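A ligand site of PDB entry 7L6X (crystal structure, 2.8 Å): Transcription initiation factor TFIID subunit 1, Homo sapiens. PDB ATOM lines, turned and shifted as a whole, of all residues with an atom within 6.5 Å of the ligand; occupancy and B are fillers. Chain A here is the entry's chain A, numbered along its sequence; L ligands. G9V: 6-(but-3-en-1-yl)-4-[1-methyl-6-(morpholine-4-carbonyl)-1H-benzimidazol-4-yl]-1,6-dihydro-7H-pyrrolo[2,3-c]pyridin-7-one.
An oxygen (O15) of the ligand lies within hydrogen-bond range of the side-chain amide nitrogen of Asn 213.
O27 of the ligand lies within hydrogen-bond range of N of Asn 163.
N4 of the ligand lies within hydrogen-bond range of OH of Tyr 219, 2.9 Å away.
ND2 of Asn 213 lies within hydrogen-bond range of OG of Ser 209 (3.0 Å).
OD1 of Asn 163 lies within hydrogen-bond range of N of Lys 165 (2.8 Å).
O of Phe 158 is in hydrogen-bond range of N of Leu 180, at 2.8 Å.
Residues that only touch the ligand: Met 178 (3.0 Å), His 160 (3.4 Å), Pro 161 (3.4 Å), Val 162 (3.4 Å), Pro 157 (3.4 Å), Phe 158 (3.5 Å), Tyr 170 (3.5 Å), Phe 166 (3.7 Å), Trp 156 (3.8 Å), Tyr 212 (3.9 Å), Asp 179 (3.9 Å) and Val 167 (3.9 Å).
Of the 23 residues printed, 15 come within 4 Å of the ligand.
The nearest printed residue that does not touch the ligand is Ser 209 (4.7 Å).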
ATOM      1  N   TRP A 156      15.454   0.676  -9.442  1.00  0.00           N
ATOM      2  CA  TRP A 156      15.310   0.852  -7.987  1.00  0.00           C
ATOM      3  C   TRP A 156      15.566   2.293  -7.514  1.00  0.00           C
ATOM      4  O   TRP A 156      14.934   2.709  -6.532  1.00  0.00           O
ATOM      5  CB  TRP A 156      16.196  -0.128  -7.235  1.00  0.00           C
ATOM      6  CG  TRP A 156      17.589   0.085  -7.455  1.00  0.00           C
ATOM      7  CD1 TRP A 156      18.374  -0.548  -8.373  1.00  0.00           C
ATOM      8  CD2 TRP A 156      18.417   1.033  -6.796  1.00  0.00           C
ATOM      9  NE1 TRP A 156      19.652  -0.065  -8.302  1.00  0.00           N
ATOM     10  CE2 TRP A 156      19.710   0.908  -7.354  1.00  0.00           C
ATOM     11  CE3 TRP A 156      18.204   1.971  -5.788  1.00  0.00           C
ATOM     12  CZ2 TRP A 156      20.779   1.689  -6.920  1.00  0.00           C
ATOM     13  CZ3 TRP A 156      19.258   2.760  -5.383  1.00  0.00           C
ATOM     14  CH2 TRP A 156      20.531   2.613  -5.947  1.00  0.00           C
ATOM     15  N   PRO A 157      16.466   3.072  -8.108  1.00  0.00           N
ATOM     16  CA  PRO A 157      16.682   4.433  -7.594  1.00  0.00           C
ATOM     17  C   PRO A 157      15.441   5.310  -7.621  1.00  0.00           C
ATOM     18  O   PRO A 157      15.416   6.342  -6.949  1.00  0.00           O
ATOM     19  CB  PRO A 157      17.794   4.978  -8.496  1.00  0.00           C
ATOM     20  CG  PRO A 157      18.472   3.780  -8.995  1.00  0.00           C
ATOM     21  CD  PRO A 157      17.393   2.809  -9.223  1.00  0.00           C
ATOM     22  N   PHE A 158      14.444   4.985  -8.420  1.00  0.00           N
ATOM     23  CA  PHE A 158      13.265   5.817  -8.604  1.00  0.00           C
ATOM     24  C   PHE A 158      12.067   5.277  -7.873  1.00  0.00           C
ATOM     25  O   PHE A 158      10.978   5.840  -7.960  1.00  0.00           O
ATOM     26  CB  PHE A 158      12.941   5.908 -10.104  1.00  0.00           C
ATOM     27  CG  PHE A 158      14.088   6.338 -10.952  1.00  0.00           C
ATOM     28  CD1 PHE A 158      14.484   7.670 -10.957  1.00  0.00           C
ATOM     29  CD2 PHE A 158      14.922   5.398 -11.522  1.00  0.00           C
ATOM     30  CE1 PHE A 158      15.549   8.072 -11.681  1.00  0.00           C
ATOM     31  CE2 PHE A 158      16.030   5.803 -12.231  1.00  0.00           C
ATOM     32  CZ  PHE A 158      16.346   7.136 -12.296  1.00  0.00           C
ATOM     33  N   HIS A 159      12.242   4.209  -7.106  1.00  0.00           N
ATOM     34  CA  HIS A 159      11.112   3.600  -6.420  1.00  0.00           C
ATOM     35  C   HIS A 159      10.682   4.394  -5.219  1.00  0.00           C
ATOM     36  O   HIS A 159       9.539   4.241  -4.784  1.00  0.00           O
ATOM     37  CB  HIS A 159      11.469   2.182  -6.009  1.00  0.00           C
ATOM     38  CG  HIS A 159      11.587   1.268  -7.177  1.00  0.00           C
ATOM     39  ND1 HIS A 159      11.376  -0.097  -7.095  1.00  0.00           N
ATOM     40  CD2 HIS A 159      11.966   1.511  -8.442  1.00  0.00           C
ATOM     41  CE1 HIS A 159      11.581  -0.634  -8.282  1.00  0.00           C
ATOM     42  NE2 HIS A 159      11.940   0.315  -9.116  1.00  0.00           N
ATOM     43  N   HIS A 160      11.568   5.201  -4.639  1.00  0.00           N
ATOM     44  CA  HIS A 160      11.215   5.833  -3.388  1.00  0.00           C
ATOM     45  C   HIS A 160      11.773   7.244  -3.431  1.00  0.00           C
ATOM     46  O   HIS A 160      12.719   7.525  -4.191  1.00  0.00           O
ATOM     47  CB  HIS A 160      11.779   5.058  -2.190  1.00  0.00           C
ATOM     48  CG  HIS A 160      11.329   3.632  -2.181  1.00  0.00           C
ATOM     49  ND1 HIS A 160      10.078   3.241  -1.756  1.00  0.00           N
ATOM     50  CD2 HIS A 160      11.996   2.504  -2.512  1.00  0.00           C
ATOM     51  CE1 HIS A 160       9.965   1.930  -1.883  1.00  0.00           C
ATOM     52  NE2 HIS A 160      11.123   1.461  -2.328  1.00  0.00           N
ATOM     53  N   PRO A 161      11.264   8.132  -2.590  1.00  0.00           N
ATOM     54  CA  PRO A 161      11.855   9.473  -2.502  1.00  0.00           C
ATOM     55  C   PRO A 161      13.306   9.415  -2.084  1.00  0.00           C
ATOM     56  O   PRO A 161      13.709   8.619  -1.236  1.00  0.00           O
ATOM     57  CB  PRO A 161      10.968  10.185  -1.484  1.00  0.00           C
ATOM     58  CG  PRO A 161       9.728   9.333  -1.383  1.00  0.00           C
ATOM     59  CD  PRO A 161      10.082   7.950  -1.743  1.00  0.00           C
ATOM     60  N   VAL A 162      14.068  10.316  -2.668  1.00  0.00           N
ATOM     61  CA  VAL A 162      15.463  10.413  -2.294  1.00  0.00           C
ATOM     62  C   VAL A 162      15.556  10.727  -0.820  1.00  0.00           C
ATOM     63  O   VAL A 162      14.850  11.603  -0.305  1.00  0.00           O
ATOM     64  CB  VAL A 162      16.145  11.484  -3.151  1.00  0.00           C
ATOM     65  CG1 VAL A 162      17.535  11.809  -2.650  1.00  0.00           C
ATOM     66  CG2 VAL A 162      16.176  11.051  -4.583  1.00  0.00           C
ATOM     67  N   ASN A 163      16.425  10.013  -0.145  1.00  0.00           N
ATOM     68  CA  ASN A 163      16.763  10.257   1.238  1.00  0.00           C
ATOM     69  C   ASN A 163      17.932  11.221   1.251  1.00  0.00           C
ATOM     70  O   ASN A 163      19.027  10.886   0.776  1.00  0.00           O
ATOM     71  CB  ASN A 163      17.108   8.989   1.985  1.00  0.00           C
ATOM     72  CG  ASN A 163      17.217   9.224   3.462  1.00  0.00           C
ATOM     73  OD1 ASN A 163      17.691  10.285   3.889  1.00  0.00           O
ATOM     74  ND2 ASN A 163      16.801   8.257   4.244  1.00  0.00           N
ATOM     75  N   LYS A 164      17.707  12.413   1.799  1.00  0.00           N
ATOM     76  CA  LYS A 164      18.740  13.427   1.797  1.00  0.00           C
ATOM     77  C   LYS A 164      20.002  12.910   2.474  1.00  0.00           C
ATOM     78  O   LYS A 164      21.117  13.412   2.202  1.00  0.00           O
ATOM     79  CB  LYS A 164      18.177  14.673   2.479  1.00  0.00           C
ATOM     80  CG  LYS A 164      19.043  15.910   2.536  1.00  0.00           C
ATOM     81  CD  LYS A 164      18.254  17.021   3.209  1.00  0.00           C
ATOM     82  CE  LYS A 164      19.046  18.348   3.351  1.00  0.00           C
ATOM     83  NZ  LYS A 164      18.172  19.393   4.040  1.00  0.00           N
ATOM     84  N   LYS A 165      19.862  11.896   3.322  1.00  0.00           N
ATOM     85  CA  LYS A 165      21.004  11.289   3.972  1.00  0.00           C
ATOM     86  C   LYS A 165      22.008  10.707   2.980  1.00  0.00           C
ATOM     87  O   LYS A 165      23.222  10.773   3.209  1.00  0.00           O
ATOM     88  CB  LYS A 165      20.461  10.277   4.978  1.00  0.00           C
ATOM     89  CG  LYS A 165      21.416   9.640   5.859  1.00  0.00           C
ATOM     90  CD  LYS A 165      20.669   8.732   6.825  1.00  0.00           C
ATOM     91  CE  LYS A 165      19.749   9.587   7.747  1.00  0.00           C
ATOM     92  NZ  LYS A 165      20.358   9.949   9.094  1.00  0.00           N
ATOM     93  N   PHE A 166      21.536  10.147   1.860  1.00  0.00           N
ATOM     94  CA  PHE A 166      22.426   9.498   0.888  1.00  0.00           C
ATOM     95  C   PHE A 166      22.852  10.372  -0.284  1.00  0.00           C
ATOM     96  O   PHE A 166      23.926  10.151  -0.855  1.00  0.00           O
ATOM     97  CB  PHE A 166      21.779   8.235   0.306  1.00  0.00           C
ATOM     98  CG  PHE A 166      21.418   7.215   1.307  1.00  0.00           C
ATOM     99  CD1 PHE A 166      22.249   6.985   2.410  1.00  0.00           C
ATOM    100  CD2 PHE A 166      20.286   6.445   1.144  1.00  0.00           C
ATOM    101  CE1 PHE A 166      21.929   6.015   3.362  1.00  0.00           C
ATOM    102  CE2 PHE A 166      19.954   5.463   2.078  1.00  0.00           C
ATOM    103  CZ  PHE A 166      20.775   5.253   3.191  1.00  0.00           C
ATOM    104  N   VAL A 167      22.075  11.384  -0.618  1.00  0.00           N
ATOM    105  CA  VAL A 167      22.340  12.333  -1.682  1.00  0.00           C
ATOM    106  C   VAL A 167      22.193  13.714  -1.077  1.00  0.00           C
ATOM    107  O   VAL A 167      21.128  14.328  -1.192  1.00  0.00           O
ATOM    108  CB  VAL A 167      21.370  12.158  -2.859  1.00  0.00           C
ATOM    109  CG1 VAL A 167      21.848  12.985  -4.046  1.00  0.00           C
ATOM    110  CG2 VAL A 167      21.214  10.650  -3.230  1.00  0.00           C
ATOM    111  N   TYR A 170      20.504  16.830  -3.005  1.00  0.00           N
ATOM    112  CA  TYR A 170      19.487  16.620  -4.032  1.00  0.00           C
ATOM    113  C   TYR A 170      18.386  17.681  -4.000  1.00  0.00           C
ATOM    114  O   TYR A 170      18.069  18.282  -5.029  1.00  0.00           O
ATOM    115  CB  TYR A 170      18.869  15.224  -3.840  1.00  0.00           C
ATOM    116  CG  TYR A 170      17.908  14.803  -4.921  1.00  0.00           C
ATOM    117  CD1 TYR A 170      18.391  14.403  -6.156  1.00  0.00           C
ATOM    118  CD2 TYR A 170      16.532  14.772  -4.715  1.00  0.00           C
ATOM    119  CE1 TYR A 170      17.543  13.996  -7.143  1.00  0.00           C
ATOM    120  CE2 TYR A 170      15.675  14.375  -5.701  1.00  0.00           C
ATOM    121  CZ  TYR A 170      16.188  13.986  -6.931  1.00  0.00           C
ATOM    122  OH  TYR A 170      15.353  13.587  -7.971  1.00  0.00           O
ATOM    123  N   PRO A 177      10.492  17.387  -6.696  1.00  0.00           N
ATOM    124  CA  PRO A 177      10.932  15.992  -6.683  1.00  0.00           C
ATOM    125  C   PRO A 177       9.752  15.089  -7.022  1.00  0.00           C
ATOM    126  O   PRO A 177       8.587  15.433  -6.821  1.00  0.00           O
ATOM    127  CB  PRO A 177      11.367  15.765  -5.241  1.00  0.00           C
ATOM    128  CG  PRO A 177      10.528  16.674  -4.506  1.00  0.00           C
ATOM    129  CD  PRO A 177      10.395  17.922  -5.332  1.00  0.00           C
ATOM    130  N   MET A 178      10.079  13.925  -7.555  1.00  0.00           N
ATOM    131  CA  MET A 178       9.040  12.953  -7.859  1.00  0.00           C
ATOM    132  C   MET A 178       9.657  11.568  -7.872  1.00  0.00           C
ATOM    133  O   MET A 178      10.856  11.425  -8.112  1.00  0.00           O
ATOM    134  CB  MET A 178       8.419  13.252  -9.229  1.00  0.00           C
ATOM    135  CG  MET A 178       7.156  12.492  -9.597  1.00  0.00           C
ATOM    136  SD  MET A 178       5.838  12.464  -8.367  1.00  0.00           S
ATOM    137  CE  MET A 178       5.494  14.211  -8.134  1.00  0.00           C
ATOM    138  N   ASP A 179       8.842  10.557  -7.557  1.00  0.00           N
ATOM    139  CA  ASP A 179       9.286   9.164  -7.514  1.00  0.00           C
ATOM    140  C   ASP A 179       8.099   8.208  -7.717  1.00  0.00           C
ATOM    141  O   ASP A 179       6.929   8.614  -7.661  1.00  0.00           O
ATOM    142  CB  ASP A 179       9.982   8.837  -6.193  1.00  0.00           C
ATOM    143  CG  ASP A 179       9.049   8.983  -5.029  1.00  0.00           C
ATOM    144  OD1 ASP A 179       8.979  10.114  -4.489  1.00  0.00           O
ATOM    145  OD2 ASP A 179       8.330   8.007  -4.730  1.00  0.00           O
ATOM    146  N   LEU A 180       8.408   6.922  -7.926  1.00  0.00           N
ATOM    147  CA  LEU A 180       7.304   6.015  -8.235  1.00  0.00           C
ATOM    148  C   LEU A 180       6.413   5.745  -7.018  1.00  0.00           C
ATOM    149  O   LEU A 180       5.193   5.642  -7.173  1.00  0.00           O
ATOM    150  CB  LEU A 180       7.842   4.685  -8.776  1.00  0.00           C
ATOM    151  CG  LEU A 180       8.616   4.739 -10.114  1.00  0.00           C
ATOM    152  CD1 LEU A 180       9.239   3.410 -10.556  1.00  0.00           C
ATOM    153  CD2 LEU A 180       7.796   5.312 -11.211  1.00  0.00           C
ATOM    154  N   ILE A 205       9.922  12.901 -13.536  1.00  0.00           N
ATOM    155  CA  ILE A 205      11.049  12.035 -13.170  1.00  0.00           C
ATOM    156  C   ILE A 205      12.195  12.146 -14.159  1.00  0.00           C
ATOM    157  O   ILE A 205      13.362  12.338 -13.779  1.00  0.00           O
ATOM    158  CB  ILE A 205      10.598  10.587 -13.038  1.00  0.00           C
ATOM    159  CG1 ILE A 205       9.571  10.471 -11.925  1.00  0.00           C
ATOM    160  CG2 ILE A 205      11.759   9.678 -12.937  1.00  0.00           C
ATOM    161  CD1 ILE A 205       9.053   9.108 -11.799  1.00  0.00           C
ATOM    162  N   ASN A 208      13.887  15.585 -13.984  1.00  0.00           N
ATOM    163  CA  ASN A 208      14.745  15.721 -12.828  1.00  0.00           C
ATOM    164  C   ASN A 208      16.020  14.937 -12.944  1.00  0.00           C
ATOM    165  O   ASN A 208      17.083  15.426 -12.530  1.00  0.00           O
ATOM    166  CB  ASN A 208      14.031  15.243 -11.592  1.00  0.00           C
ATOM    167  CG  ASN A 208      12.932  16.145 -11.195  1.00  0.00           C
ATOM    168  OD1 ASN A 208      12.901  17.317 -11.554  1.00  0.00           O
ATOM    169  ND2 ASN A 208      11.981  15.592 -10.437  1.00  0.00           N
ATOM    170  N   SER A 209      15.975  13.782 -13.588  1.00  0.00           N
ATOM    171  CA  SER A 209      17.222  13.065 -13.734  1.00  0.00           C
ATOM    172  C   SER A 209      18.160  13.809 -14.636  1.00  0.00           C
ATOM    173  O   SER A 209      19.369  13.857 -14.374  1.00  0.00           O
ATOM    174  CB  SER A 209      17.008  11.655 -14.256  1.00  0.00           C
ATOM    175  OG  SER A 209      18.261  10.987 -14.265  1.00  0.00           O
ATOM    176  N   TYR A 212      19.742  16.645 -12.471  1.00  0.00           N
ATOM    177  CA  TYR A 212      20.657  16.308 -11.392  1.00  0.00           C
ATOM    178  C   TYR A 212      21.831  15.476 -11.875  1.00  0.00           C
ATOM    179  O   TYR A 212      22.955  15.690 -11.431  1.00  0.00           O
ATOM    180  CB  TYR A 212      19.945  15.574 -10.250  1.00  0.00           C
ATOM    181  CG  TYR A 212      20.880  15.366  -9.052  1.00  0.00           C
ATOM    182  CD1 TYR A 212      21.742  14.274  -8.997  1.00  0.00           C
ATOM    183  CD2 TYR A 212      21.017  16.338  -8.054  1.00  0.00           C
ATOM    184  CE1 TYR A 212      22.665  14.097  -7.941  1.00  0.00           C
ATOM    185  CE2 TYR A 212      21.929  16.181  -6.988  1.00  0.00           C
ATOM    186  CZ  TYR A 212      22.753  15.056  -6.936  1.00  0.00           C
ATOM    187  OH  TYR A 212      23.653  14.877  -5.896  1.00  0.00           O
ATOM    188  N   ASN A 213      21.594  14.534 -12.780  1.00  0.00           N
ATOM    189  CA  ASN A 213      22.612  13.584 -13.202  1.00  0.00           C
ATOM    190  C   ASN A 213      23.273  13.945 -14.504  1.00  0.00           C
ATOM    191  O   ASN A 213      24.388  13.474 -14.750  1.00  0.00           O
ATOM    192  CB  ASN A 213      22.011  12.191 -13.316  1.00  0.00           C
ATOM    193  CG  ASN A 213      21.458  11.718 -12.012  1.00  0.00           C
ATOM    194  OD1 ASN A 213      22.174  11.686 -10.997  1.00  0.00           O
ATOM    195  ND2 ASN A 213      20.184  11.463 -11.967  1.00  0.00           N
ATOM    196  N   TYR A 219      21.605   7.145 -14.838  1.00  0.00           N
ATOM    197  CA  TYR A 219      20.304   7.394 -14.216  1.00  0.00           C
ATOM    198  C   TYR A 219      19.295   7.866 -15.260  1.00  0.00           C
ATOM    199  O   TYR A 219      18.170   7.353 -15.341  1.00  0.00           O
ATOM    200  CB  TYR A 219      20.424   8.431 -13.100  1.00  0.00           C
ATOM    201  CG  TYR A 219      21.120   7.970 -11.840  1.00  0.00           C
ATOM    202  CD1 TYR A 219      20.528   7.045 -10.995  1.00  0.00           C
ATOM    203  CD2 TYR A 219      22.376   8.457 -11.493  1.00  0.00           C
ATOM    204  CE1 TYR A 219      21.165   6.604  -9.850  1.00  0.00           C
ATOM    205  CE2 TYR A 219      23.010   8.024 -10.369  1.00  0.00           C
ATOM    206  CZ  TYR A 219      22.405   7.098  -9.542  1.00  0.00           C
ATOM    207  OH  TYR A 219      23.044   6.657  -8.388  1.00  0.00           O
HETATM  208  C7  G9V L   1      20.231   5.906  -2.678  1.00  0.00           C
HETATM  209  C9  G9V L   1      18.988   7.468  -4.046  1.00  0.00           C
HETATM  210  N2  G9V L   1      22.350   5.121  -3.813  1.00  0.00           N
HETATM  211  C10 G9V L   1      19.929   7.383  -5.064  1.00  0.00           C
HETATM  212  C6  G9V L   1      21.200   5.822  -3.709  1.00  0.00           C
HETATM  213  C29 G9V L   1      16.328   5.781  -0.460  1.00  0.00           C
HETATM  214  N20 G9V L   1      21.689  10.382  -8.522  1.00  0.00           N
HETATM  215  C18 G9V L   1      22.142   9.183  -6.723  1.00  0.00           C
HETATM  216  C11 G9V L   1      19.708   8.218  -6.314  1.00  0.00           C
HETATM  217  C1  G9V L   1      22.894   4.223  -2.806  1.00  0.00           C
HETATM  218  C8  G9V L   1      19.149   6.734  -2.885  1.00  0.00           C
HETATM  219  C16 G9V L   1      20.551   9.777  -8.098  1.00  0.00           C
HETATM  220  C5  G9V L   1      21.059   6.547  -4.872  1.00  0.00           C
HETATM  221  O15 G9V L   1      18.958  10.481  -9.653  1.00  0.00           O
HETATM  222  N13 G9V L   1      18.065   9.087  -8.076  1.00  0.00           N
HETATM  223  C24 G9V L   1      14.469   9.497  -7.861  1.00  0.00           C
HETATM  224  C25 G9V L   1      13.434  10.157  -7.396  1.00  0.00           C
HETATM  225  C32 G9V L   1      16.110   4.199  -2.690  1.00  0.00           C
HETATM  226  C17 G9V L   1      20.809   9.017  -6.979  1.00  0.00           C
HETATM  227  C22 G9V L   1      16.748   9.146  -8.623  1.00  0.00           C
HETATM  228  O31 G9V L   1      15.021   4.309  -1.775  1.00  0.00           O
HETATM  229  C12 G9V L   1      18.325   8.280  -6.893  1.00  0.00           C
HETATM  230  C19 G9V L   1      22.681  10.037  -7.686  1.00  0.00           C
HETATM  231  C14 G9V L   1      19.137   9.827  -8.692  1.00  0.00           C
HETATM  232  N28 G9V L   1      17.353   5.722  -1.450  1.00  0.00           N
HETATM  233  C33 G9V L   1      17.468   4.431  -2.026  1.00  0.00           C
HETATM  234  C3  G9V L   1      22.901   5.390  -5.002  1.00  0.00           C
HETATM  235  C23 G9V L   1      15.867  10.087  -7.814  1.00  0.00           C
HETATM  236  C26 G9V L   1      18.100   6.875  -1.826  1.00  0.00           C
HETATM  237  C30 G9V L   1      14.972   5.512  -1.061  1.00  0.00           C
HETATM  238  O27 G9V L   1      17.890   7.926  -1.302  1.00  0.00           O
HETATM  239  N4  G9V L   1      22.139   6.264  -5.642  1.00  0.00           N
